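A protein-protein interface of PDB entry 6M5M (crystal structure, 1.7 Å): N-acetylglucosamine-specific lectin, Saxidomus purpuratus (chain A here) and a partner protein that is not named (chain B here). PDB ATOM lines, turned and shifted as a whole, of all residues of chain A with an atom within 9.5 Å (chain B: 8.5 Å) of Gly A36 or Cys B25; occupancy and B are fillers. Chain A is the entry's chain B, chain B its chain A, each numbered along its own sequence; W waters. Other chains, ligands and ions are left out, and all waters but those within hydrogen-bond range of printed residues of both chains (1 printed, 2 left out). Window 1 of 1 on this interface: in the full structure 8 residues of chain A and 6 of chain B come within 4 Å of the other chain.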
ATOM      1  N   CYS A  22      12.428  18.970  23.828  1.00  0.00           N
ATOM      2  CA  CYS A  22      11.128  18.801  24.506  1.00  0.00           C
ATOM      3  C   CYS A  22      11.267  19.036  26.022  1.00  0.00           C
ATOM      4  O   CYS A  22      11.987  18.291  26.694  1.00  0.00           O
ATOM      5  CB  CYS A  22      10.552  17.420  24.204  1.00  0.00           C
ATOM      6  SG  CYS A  22      10.166  17.190  22.445  1.00  0.00           S
ATOM      7  N   CYS A  23      10.614  20.068  26.543  1.00  0.00           N
ATOM      8  CA  CYS A  23      10.539  20.358  27.996  1.00  0.00           C
ATOM      9  C   CYS A  23       9.524  19.449  28.686  1.00  0.00           C
ATOM     10  O   CYS A  23       8.582  18.982  27.997  1.00  0.00           O
ATOM     11  CB  CYS A  23      10.070  21.780  28.254  1.00  0.00           C
ATOM     12  SG  CYS A  23      10.925  22.977  27.205  1.00  0.00           S
ATOM     13  N   SER A  24       9.674  19.280  30.009  1.00  0.00           N
ATOM     14  CA  SER A  24       8.599  18.812  30.928  1.00  0.00           C
ATOM     15  C   SER A  24       8.046  20.006  31.708  1.00  0.00           C
ATOM     16  O   SER A  24       8.659  21.074  31.660  1.00  0.00           O
ATOM     17  CB  SER A  24       9.087  17.725  31.865  1.00  0.00           C
ATOM     18  OG  SER A  24      10.313  18.105  32.474  1.00  0.00           O
ATOM     19  N   GLU A  25       6.916  19.814  32.395  1.00  0.00           N
ATOM     20  CA  GLU A  25       6.258  20.836  33.249  1.00  0.00           C
ATOM     21  C   GLU A  25       7.321  21.422  34.197  1.00  0.00           C
ATOM     22  O   GLU A  25       7.356  22.662  34.356  1.00  0.00           O
ATOM     23  CB  GLU A  25       5.041  20.226  33.956  1.00  0.00           C
ATOM     24  CG  GLU A  25       4.345  21.191  34.903  1.00  0.00           C
ATOM     25  CD  GLU A  25       2.839  21.020  35.063  1.00  0.00           C
ATOM     26  OE1 GLU A  25       2.137  22.050  35.201  1.00  0.00           O
ATOM     27  OE2 GLU A  25       2.366  19.864  35.074  1.00  0.00           O
ATOM     28  N   CYS A  28       9.297  24.650  32.986  1.00  0.00           N
ATOM     29  CA  CYS A  28       8.564  25.939  32.832  1.00  0.00           C
ATOM     30  C   CYS A  28       8.861  26.878  34.005  1.00  0.00           C
ATOM     31  O   CYS A  28       8.446  26.608  35.142  1.00  0.00           O
ATOM     32  CB  CYS A  28       7.064  25.703  32.684  1.00  0.00           C
ATOM     33  SG  CYS A  28       6.668  24.812  31.156  1.00  0.00           S
ATOM     34  N   LYS A  33       3.239  28.652  31.007  1.00  0.00           N
ATOM     35  CA  LYS A  33       2.306  27.513  30.855  1.00  0.00           C
ATOM     36  C   LYS A  33       2.965  26.387  30.067  1.00  0.00           C
ATOM     37  O   LYS A  33       3.583  26.664  29.025  1.00  0.00           O
ATOM     38  CB  LYS A  33       1.044  27.945  30.104  1.00  0.00           C
ATOM     39  CG  LYS A  33       0.340  29.127  30.758  1.00  0.00           C
ATOM     40  CD  LYS A  33      -0.969  29.519  30.139  1.00  0.00           C
ATOM     41  CE  LYS A  33      -1.417  30.907  30.549  1.00  0.00           C
ATOM     42  NZ  LYS A  33      -1.928  30.910  31.943  1.00  0.00           N
ATOM     43  N   PHE A  34       2.783  25.153  30.523  1.00  0.00           N
ATOM     44  CA  PHE A  34       3.297  23.952  29.835  1.00  0.00           C
ATOM     45  C   PHE A  34       2.269  23.443  28.834  1.00  0.00           C
ATOM     46  O   PHE A  34       1.087  23.305  29.198  1.00  0.00           O
ATOM     47  CB  PHE A  34       3.611  22.839  30.833  1.00  0.00           C
ATOM     48  CG  PHE A  34       4.109  21.598  30.141  1.00  0.00           C
ATOM     49  CD1 PHE A  34       5.378  21.569  29.579  1.00  0.00           C
ATOM     50  CD2 PHE A  34       3.291  20.484  29.990  1.00  0.00           C
ATOM     51  CE1 PHE A  34       5.833  20.431  28.924  1.00  0.00           C
ATOM     52  CE2 PHE A  34       3.745  19.353  29.320  1.00  0.00           C
ATOM     53  CZ  PHE A  34       5.008  19.338  28.774  1.00  0.00           C
ATOM     54  N   PHE A  35       2.715  23.116  27.625  1.00  0.00           N
ATOM     55  CA  PHE A  35       1.914  22.372  26.621  1.00  0.00           C
ATOM     56  C   PHE A  35       2.802  21.681  25.594  1.00  0.00           C
ATOM     57  O   PHE A  35       3.692  22.317  25.067  1.00  0.00           O
ATOM     58  CB  PHE A  35       0.982  23.277  25.823  1.00  0.00           C
ATOM     59  CG  PHE A  35       0.185  22.468  24.842  1.00  0.00           C
ATOM     60  CD1 PHE A  35      -0.916  21.742  25.275  1.00  0.00           C
ATOM     61  CD2 PHE A  35       0.586  22.345  23.517  1.00  0.00           C
ATOM     62  CE1 PHE A  35      -1.648  20.965  24.389  1.00  0.00           C
ATOM     63  CE2 PHE A  35      -0.133  21.550  22.633  1.00  0.00           C
ATOM     64  CZ  PHE A  35      -1.245  20.864  23.068  1.00  0.00           C
ATOM     65  N   GLY A  36       2.505  20.424  25.258  1.00  0.00           N
ATOM     66  CA  GLY A  36       3.149  19.756  24.115  1.00  0.00           C
ATOM     67  C   GLY A  36       4.660  19.892  24.121  1.00  0.00           C
ATOM     68  O   GLY A  36       5.260  20.167  23.060  1.00  0.00           O
ATOM     69  N   GLY A  37       5.281  19.724  25.283  1.00  0.00           N
ATOM     70  CA  GLY A  37       6.754  19.752  25.402  1.00  0.00           C
ATOM     71  C   GLY A  37       7.351  21.140  25.188  1.00  0.00           C
ATOM     72  O   GLY A  37       8.576  21.270  24.917  1.00  0.00           O
ATOM     73  N   SER A  38       6.538  22.165  25.372  1.00  0.00           N
ATOM     74  CA  SER A  38       6.957  23.578  25.326  1.00  0.00           C
ATOM     75  C   SER A  38       6.456  24.288  26.572  1.00  0.00           C
ATOM     76  O   SER A  38       5.369  23.877  27.112  1.00  0.00           O
ATOM     77  CB  SER A  38       6.433  24.223  24.067  1.00  0.00           C
ATOM     78  OG  SER A  38       7.206  23.791  22.965  1.00  0.00           O
ATOM     79  N   CYS A  39       7.191  25.343  26.939  1.00  0.00           N
ATOM     80  CA  CYS A  39       6.833  26.348  27.972  1.00  0.00           C
ATOM     81  C   CYS A  39       6.480  27.671  27.280  1.00  0.00           C
ATOM     82  O   CYS A  39       7.267  28.152  26.476  1.00  0.00           O
ATOM     83  CB  CYS A  39       7.996  26.527  28.940  1.00  0.00           C
ATOM     84  SG  CYS A  39       8.329  25.009  29.881  1.00  0.00           S
ATOM     85  N   TYR A  40       5.331  28.236  27.612  1.00  0.00           N
ATOM     86  CA  TYR A  40       4.835  29.456  26.948  1.00  0.00           C
ATOM     87  C   TYR A  40       4.662  30.584  27.966  1.00  0.00           C
ATOM     88  O   TYR A  40       4.082  30.372  29.074  1.00  0.00           O
ATOM     89  CB  TYR A  40       3.516  29.157  26.247  1.00  0.00           C
ATOM     90  CG  TYR A  40       3.591  28.064  25.210  1.00  0.00           C
ATOM     91  CD1 TYR A  40       3.518  26.729  25.550  1.00  0.00           C
ATOM     92  CD2 TYR A  40       3.736  28.380  23.873  1.00  0.00           C
ATOM     93  CE1 TYR A  40       3.594  25.734  24.594  1.00  0.00           C
ATOM     94  CE2 TYR A  40       3.798  27.398  22.903  1.00  0.00           C
ATOM     95  CZ  TYR A  40       3.720  26.072  23.260  1.00  0.00           C
ATOM     96  OH  TYR A  40       3.814  25.108  22.307  1.00  0.00           O
ATOM     97  N   THR A  65       6.638  29.626  17.803  1.00  0.00           N
ATOM     98  CA  THR A  65       6.582  28.976  16.456  1.00  0.00           C
ATOM     99  C   THR A  65       5.577  27.833  16.603  1.00  0.00           C
ATOM    100  O   THR A  65       5.616  27.126  17.642  1.00  0.00           O
ATOM    101  CB  THR A  65       7.975  28.533  15.984  1.00  0.00           C
ATOM    102  OG1 THR A  65       8.510  27.579  16.911  1.00  0.00           O
ATOM    103  CG2 THR A  65       8.939  29.689  15.824  1.00  0.00           C
ATOM    104  N   GLU A  67       3.929  24.527  15.084  1.00  0.00           N
ATOM    105  CA  GLU A  67       4.360  23.475  14.128  1.00  0.00           C
ATOM    106  C   GLU A  67       3.195  22.546  13.790  1.00  0.00           C
ATOM    107  O   GLU A  67       3.328  21.814  12.793  1.00  0.00           O
ATOM    108  CB  GLU A  67       5.569  22.760  14.734  1.00  0.00           C
ATOM    109  CG  GLU A  67       6.857  23.585  14.601  1.00  0.00           C
ATOM    110  CD  GLU A  67       7.182  24.465  15.811  1.00  0.00           C
ATOM    111  OE1 GLU A  67       6.501  24.301  16.852  1.00  0.00           O
ATOM    112  OE2 GLU A  67       8.119  25.285  15.711  1.00  0.00           O
ATOM    113  N   CYS A  68       2.115  22.560  14.574  1.00  0.00           N
ATOM    114  CA  CYS A  68       0.977  21.630  14.432  1.00  0.00           C
ATOM    115  C   CYS A  68      -0.325  22.210  14.978  1.00  0.00           C
ATOM    116  O   CYS A  68      -0.311  23.232  15.728  1.00  0.00           O
ATOM    117  CB  CYS A  68       1.264  20.333  15.177  1.00  0.00           C
ATOM    118  SG  CYS A  68       1.313  20.558  16.979  1.00  0.00           S
ATOM    119  N   LYS A  70      -2.411  21.076  17.163  1.00  0.00           N
ATOM    120  CA  LYS A  70      -2.713  20.972  18.625  1.00  0.00           C
ATOM    121  C   LYS A  70      -2.147  22.193  19.354  1.00  0.00           C
ATOM    122  O   LYS A  70      -2.772  22.665  20.348  1.00  0.00           O
ATOM    123  CB  LYS A  70      -2.175  19.664  19.199  1.00  0.00           C
ATOM    124  CG  LYS A  70      -3.143  18.490  19.115  1.00  0.00           C
ATOM    125  CD  LYS A  70      -2.583  17.258  19.806  1.00  0.00           C
ATOM    126  CE  LYS A  70      -1.691  16.468  18.881  1.00  0.00           C
ATOM    127  NZ  LYS A  70      -0.629  15.749  19.626  1.00  0.00           N
ATOM    128  N   GLU A  71      -0.974  22.657  18.911  1.00  0.00           N
ATOM    129  CA  GLU A  71      -0.300  23.854  19.476  1.00  0.00           C
ATOM    130  C   GLU A  71      -1.113  25.102  19.137  1.00  0.00           C
ATOM    131  O   GLU A  71      -1.237  25.967  19.990  1.00  0.00           O
ATOM    132  CB  GLU A  71       1.143  23.945  18.969  1.00  0.00           C
ATOM    133  CG  GLU A  71       1.999  24.980  19.700  1.00  0.00           C
ATOM    134  CD  GLU A  71       3.424  25.007  19.203  1.00  0.00           C
ATOM    135  OE1 GLU A  71       3.626  24.506  18.091  1.00  0.00           O
ATOM    136  OE2 GLU A  71       4.350  25.538  19.904  1.00  0.00           O
ATOM    137  N   PHE A  74      -4.122  25.003  21.376  1.00  0.00           N
ATOM    138  CA  PHE A  74      -3.664  25.368  22.734  1.00  0.00           C
ATOM    139  C   PHE A  74      -3.684  26.888  22.831  1.00  0.00           C
ATOM    140  O   PHE A  74      -4.425  27.457  23.684  1.00  0.00           O
ATOM    141  CB  PHE A  74      -2.280  24.830  23.082  1.00  0.00           C
ATOM    142  CG  PHE A  74      -1.708  25.450  24.326  1.00  0.00           C
ATOM    143  CD1 PHE A  74      -2.258  25.167  25.565  1.00  0.00           C
ATOM    144  CD2 PHE A  74      -0.635  26.323  24.251  1.00  0.00           C
ATOM    145  CE1 PHE A  74      -1.762  25.781  26.695  1.00  0.00           C
ATOM    146  CE2 PHE A  74      -0.133  26.930  25.382  1.00  0.00           C
ATOM    147  CZ  PHE A  74      -0.696  26.647  26.604  1.00  0.00           C
ATOM    148  N   GLU A 154       8.155  31.343  23.647  1.00  0.00           N
ATOM    149  CA  GLU A 154       8.191  29.866  23.769  1.00  0.00           C
ATOM    150  C   GLU A 154       9.619  29.405  24.086  1.00  0.00           C
ATOM    151  O   GLU A 154      10.526  29.834  23.389  1.00  0.00           O
ATOM    152  CB  GLU A 154       7.649  29.265  22.463  1.00  0.00           C
ATOM    153  CG  GLU A 154       7.566  27.742  22.495  1.00  0.00           C
ATOM    154  CD  GLU A 154       7.375  27.052  21.147  1.00  0.00           C
ATOM    155  OE1 GLU A 154       7.527  27.753  20.090  1.00  0.00           O
ATOM    156  OE2 GLU A 154       7.165  25.794  21.155  1.00  0.00           O
ATOM    157  N   ILE A 155       9.757  28.470  25.026  1.00  0.00           N
ATOM    158  CA  ILE A 155      10.985  27.672  25.296  1.00  0.00           C
ATOM    159  C   ILE A 155      10.602  26.224  24.977  1.00  0.00           C
ATOM    160  O   ILE A 155       9.639  25.727  25.623  1.00  0.00           O
ATOM    161  CB  ILE A 155      11.469  27.851  26.764  1.00  0.00           C
ATOM    162  CG1 ILE A 155      11.640  29.322  27.167  1.00  0.00           C
ATOM    163  CG2 ILE A 155      12.773  27.085  27.001  1.00  0.00           C
ATOM    164  CD1 ILE A 155      11.785  29.563  28.675  1.00  0.00           C
ATOM    165  N   ASP A 156      11.251  25.577  23.998  1.00  0.00           N
ATOM    166  CA  ASP A 156      10.846  24.213  23.552  1.00  0.00           C
ATOM    167  C   ASP A 156      11.968  23.207  23.861  1.00  0.00           C
ATOM    168  O   ASP A 156      11.772  22.000  23.561  1.00  0.00           O
ATOM    169  CB  ASP A 156      10.347  24.262  22.097  1.00  0.00           C
ATOM    170  CG  ASP A 156      11.432  24.504  21.051  1.00  0.00           C
ATOM    171  OD1 ASP A 156      12.610  24.663  21.447  1.00  0.00           O
ATOM    172  OD2 ASP A 156      11.085  24.509  19.831  1.00  0.00           O
ATOM    173  N   CYS A 157      13.050  23.670  24.510  1.00  0.00           N
ATOM    174  CA  CYS A 157      14.168  22.852  25.069  1.00  0.00           C
ATOM    175  C   CYS A 157      14.832  22.017  23.969  1.00  0.00           C
ATOM    176  O   CYS A 157      15.225  20.888  24.268  1.00  0.00           O
ATOM    177  CB  CYS A 157      13.688  21.909  26.168  1.00  0.00           C
ATOM    178  SG  CYS A 157      12.947  22.737  27.602  1.00  0.00           S
ATOM    179  N   SER A 158      14.942  22.553  22.750  1.00  0.00           N
ATOM    180  CA  SER A 158      15.565  21.897  21.569  1.00  0.00           C
ATOM    181  C   SER A 158      16.954  22.488  21.318  1.00  0.00           C
ATOM    182  O   SER A 158      17.908  21.728  21.275  1.00  0.00           O
ATOM    183  CB  SER A 158      14.683  22.032  20.356  1.00  0.00           C
ATOM    184  OG  SER A 158      14.698  23.365  19.851  1.00  0.00           O
ATOM    185  N   CYS B  22       2.861  16.296  12.308  1.00  0.00           N
ATOM    186  CA  CYS B  22       3.352  15.881  13.652  1.00  0.00           C
ATOM    187  C   CYS B  22       3.771  17.109  14.471  1.00  0.00           C
ATOM    188  O   CYS B  22       4.541  17.910  13.938  1.00  0.00           O
ATOM    189  CB  CYS B  22       4.583  14.984  13.548  1.00  0.00           C
ATOM    190  SG  CYS B  22       4.292  13.393  12.710  1.00  0.00           S
ATOM    191  N   CYS B  23       3.381  17.149  15.747  1.00  0.00           N
ATOM    192  CA  CYS B  23       3.927  18.099  16.760  1.00  0.00           C
ATOM    193  C   CYS B  23       5.358  17.674  17.110  1.00  0.00           C
ATOM    194  O   CYS B  23       5.685  16.462  17.000  1.00  0.00           O
ATOM    195  CB  CYS B  23       3.054  18.167  18.010  1.00  0.00           C
ATOM    196  SG  CYS B  23       1.313  18.537  17.645  1.00  0.00           S
ATOM    197  N   LYS B  24       6.196  18.649  17.435  1.00  0.00           N
ATOM    198  CA  LYS B  24       7.656  18.488  17.605  1.00  0.00           C
ATOM    199  C   LYS B  24       7.984  17.389  18.620  1.00  0.00           C
ATOM    200  O   LYS B  24       9.097  16.886  18.546  1.00  0.00           O
ATOM    201  CB  LYS B  24       8.299  19.775  18.127  1.00  0.00           C
ATOM    202  CG  LYS B  24       8.680  20.789  17.064  1.00  0.00           C
ATOM    203  CD  LYS B  24       9.690  21.832  17.527  1.00  0.00           C
ATOM    204  CE  LYS B  24      11.061  21.255  17.813  1.00  0.00           C
ATOM    205  NZ  LYS B  24      12.070  22.327  17.967  1.00  0.00           N
ATOM    206  N   CYS B  25       7.085  17.111  19.568  1.00  0.00           N
ATOM    207  CA  CYS B  25       7.295  16.153  20.686  1.00  0.00           C
ATOM    208  C   CYS B  25       6.339  14.972  20.598  1.00  0.00           C
ATOM    209  O   CYS B  25       6.079  14.365  21.633  1.00  0.00           O
ATOM    210  CB  CYS B  25       7.101  16.876  22.007  1.00  0.00           C
ATOM    211  SG  CYS B  25       8.351  18.169  22.144  1.00  0.00           S
ATOM    212  N   ASP B  26       5.851  14.651  19.403  1.00  0.00           N
ATOM    213  CA  ASP B  26       4.820  13.598  19.222  1.00  0.00           C
ATOM    214  C   ASP B  26       5.423  12.363  18.561  1.00  0.00           C
ATOM    215  O   ASP B  26       4.668  11.394  18.403  1.00  0.00           O
ATOM    216  CB  ASP B  26       3.587  14.131  18.489  1.00  0.00           C
ATOM    217  CG  ASP B  26       2.566  14.693  19.468  1.00  0.00           C
ATOM    218  OD1 ASP B  26       2.844  14.701  20.687  1.00  0.00           O
ATOM    219  OD2 ASP B  26       1.520  15.125  19.017  1.00  0.00           O
ATOM    220  N   CYS B  27       6.715  12.373  18.231  1.00  0.00           N
ATOM    221  CA  CYS B  27       7.384  11.187  17.638  1.00  0.00           C
ATOM    222  C   CYS B  27       7.544  10.103  18.699  1.00  0.00           C
ATOM    223  O   CYS B  27       8.088  10.397  19.781  1.00  0.00           O
ATOM    224  CB  CYS B  27       8.750  11.507  17.078  1.00  0.00           C
ATOM    225  SG  CYS B  27       8.696  12.783  15.812  1.00  0.00           S
ATOM    226  N   GLN B  28       7.096   8.890  18.378  1.00  0.00           N
ATOM    227  CA  GLN B  28       7.230   7.707  19.264  1.00  0.00           C
ATOM    228  C   GLN B  28       8.723   7.409  19.423  1.00  0.00           C
ATOM    229  O   GLN B  28       9.538   8.039  18.760  1.00  0.00           O
ATOM    230  CB  GLN B  28       6.422   6.532  18.702  1.00  0.00           C
ATOM    231  CG  GLN B  28       6.953   6.023  17.375  1.00  0.00           C
ATOM    232  CD  GLN B  28       6.126   4.879  16.843  1.00  0.00           C
ATOM    233  OE1 GLN B  28       5.368   4.246  17.571  1.00  0.00           O
ATOM    234  NE2 GLN B  28       6.292   4.593  15.563  1.00  0.00           N
ATOM    235  N   TRP B  33      12.067  13.931  14.879  1.00  0.00           N
ATOM    236  CA  TRP B  33      11.175  14.957  14.271  1.00  0.00           C
ATOM    237  C   TRP B  33      11.949  15.841  13.290  1.00  0.00           C
ATOM    238  O   TRP B  33      13.030  16.296  13.616  1.00  0.00           O
ATOM    239  CB  TRP B  33      10.542  15.812  15.363  1.00  0.00           C
ATOM    240  CG  TRP B  33       9.464  16.707  14.846  1.00  0.00           C
ATOM    241  CD1 TRP B  33       8.125  16.428  14.767  1.00  0.00           C
ATOM    242  CD2 TRP B  33       9.630  18.034  14.323  1.00  0.00           C
ATOM    243  NE1 TRP B  33       7.455  17.484  14.209  1.00  0.00           N
ATOM    244  CE2 TRP B  33       8.354  18.484  13.937  1.00  0.00           C
ATOM    245  CE3 TRP B  33      10.732  18.877  14.148  1.00  0.00           C
ATOM    246  CZ2 TRP B  33       8.147  19.763  13.428  1.00  0.00           C
ATOM    247  CZ3 TRP B  33      10.536  20.128  13.610  1.00  0.00           C
ATOM    248  CH2 TRP B  33       9.258  20.560  13.252  1.00  0.00           C
ATOM    249  N   CYS B  38       7.855  12.814  11.519  1.00  0.00           N
ATOM    250  CA  CYS B  38       8.703  11.892  12.306  1.00  0.00           C
ATOM    251  C   CYS B  38       9.315  10.856  11.370  1.00  0.00           C
ATOM    252  O   CYS B  38       8.591  10.344  10.518  1.00  0.00           O
ATOM    253  CB  CYS B  38       7.844  11.209  13.346  1.00  0.00           C
ATOM    254  SG  CYS B  38       7.130  12.390  14.514  1.00  0.00           S
ATOM    255  N   CYS B 156       1.799  12.138  10.762  1.00  0.00           N
ATOM    256  CA  CYS B 156       0.923  11.915  11.956  1.00  0.00           C
ATOM    257  C   CYS B 156      -0.559  12.156  11.633  1.00  0.00           C
ATOM    258  O   CYS B 156      -1.356  12.103  12.595  1.00  0.00           O
ATOM    259  CB  CYS B 156       1.308  12.781  13.154  1.00  0.00           C
ATOM    260  SG  CYS B 156       2.927  12.404  13.882  1.00  0.00           S
HETATM  261  O   HOH W   1      -1.386  18.531  15.766  1.00  0.00           O
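O of Gly A36 sits close to SG of Cys B25, 3.8 Å away. The side-chain sulfur of Cys B25 is disulfide-bonded to the side-chain sulfur of Cys A22. The side-chain sulfur (SG) of Cys B23 forms a disulfide with the side-chain sulfur (SG) of Cys A68. OD2 of Asp A156 is in salt-bridge range of NZ of Lys B24 (3.0 Å). OD1 of Asp B26 is in salt-bridge range of NZ of Lys A70 (3.8 Å). The side-chain amino group of Lys B24 lies within hydrogen-bond range of the side-chain hydroxyl of Ser A158, at 3.4 Å.
The side-chain sulfur (SG) of Cys A28 is disulfide-bonded to the side-chain sulfur (SG) of Cys A39, at 2.1 Å. The side-chain sulfur of Cys A68 sits close to the backbone NH of Lys A70. O of Asp A156 sits at hydrogen-bond distance from N of Cys A22 (3.1 Å). SG of Cys A68 lies within hydrogen-bond range of N of Glu A71 (3.7 Å). The side-chain sulfur (SG) of Cys B22 forms a disulfide with the side-chain sulfur (SG) of Cys B156. The side-chain sulfur (SG) of Cys A23 forms a disulfide with the side-chain sulfur (SG) of Cys A157, 2.1 Å away.
Gly A37 touches Cys B25 (CA to SG, 3.96 Å). Cys B23 touches Lys A70 (SG to CE, 3.9 Å).
Printed residues of chain B within 4 Å of Gly A36: Cys B25 (3.8 Å). Of chain A, only Cys A22, Gly A36 and Gly A37 come within 4 Å of Cys B25. Of the printed residues of chain B, Gly A37 touches Cys B25 (3.96 Å). Of chain A, only Lys A70 (2.3 Å) comes within 4 Å of Asp B26. Printed residues of chain B within 4 Å of Cys A22: Cys B25 (2.1 Å). Of the printed residues of chain A, Lys B24 touches Asp A156 and Ser A158. Of the printed residues of chain A, Cys B23 touches Cys A68 and Lys A70. Printed residues of chain B within 4 Å of Ser A158: Lys B24 (3.4 Å). Ser A38 touches none of the printed residues of chain B. Cys B22 touches none of the printed residues of chain A. The nearest printed residue of chain A that does not touch Cys B25 is Cys A23 (5.3 Å). The nearest printed residue of chain B that does not touch Cys A22 is Lys B24 (4.1 Å).
Of the 10 printed residues of chain B, 4 touch a printed residue of chain A. Printed residues of chain B that touch a printed residue of chain A: Cys B23, Lys B24, Cys B25 and Asp B26. Among the printed residues, 8 pairs touch across the chains. Among the printed residues, Asp or Glu carboxylates within 4 Å of a Lys or Arg side-chain nitrogen of the other chain: Lys A70 with Asp B26 (2.3 Å) and Asp A156 with Lys B24 (3.0 Å).
Water W1 lies within hydrogen-bond range of the backbone NH of Lys A70 (3.1 Å), the side-chain sulfur of Cys B23 (3.3 Å) and the side-chain sulfur of Cys A68 (3.6 Å).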
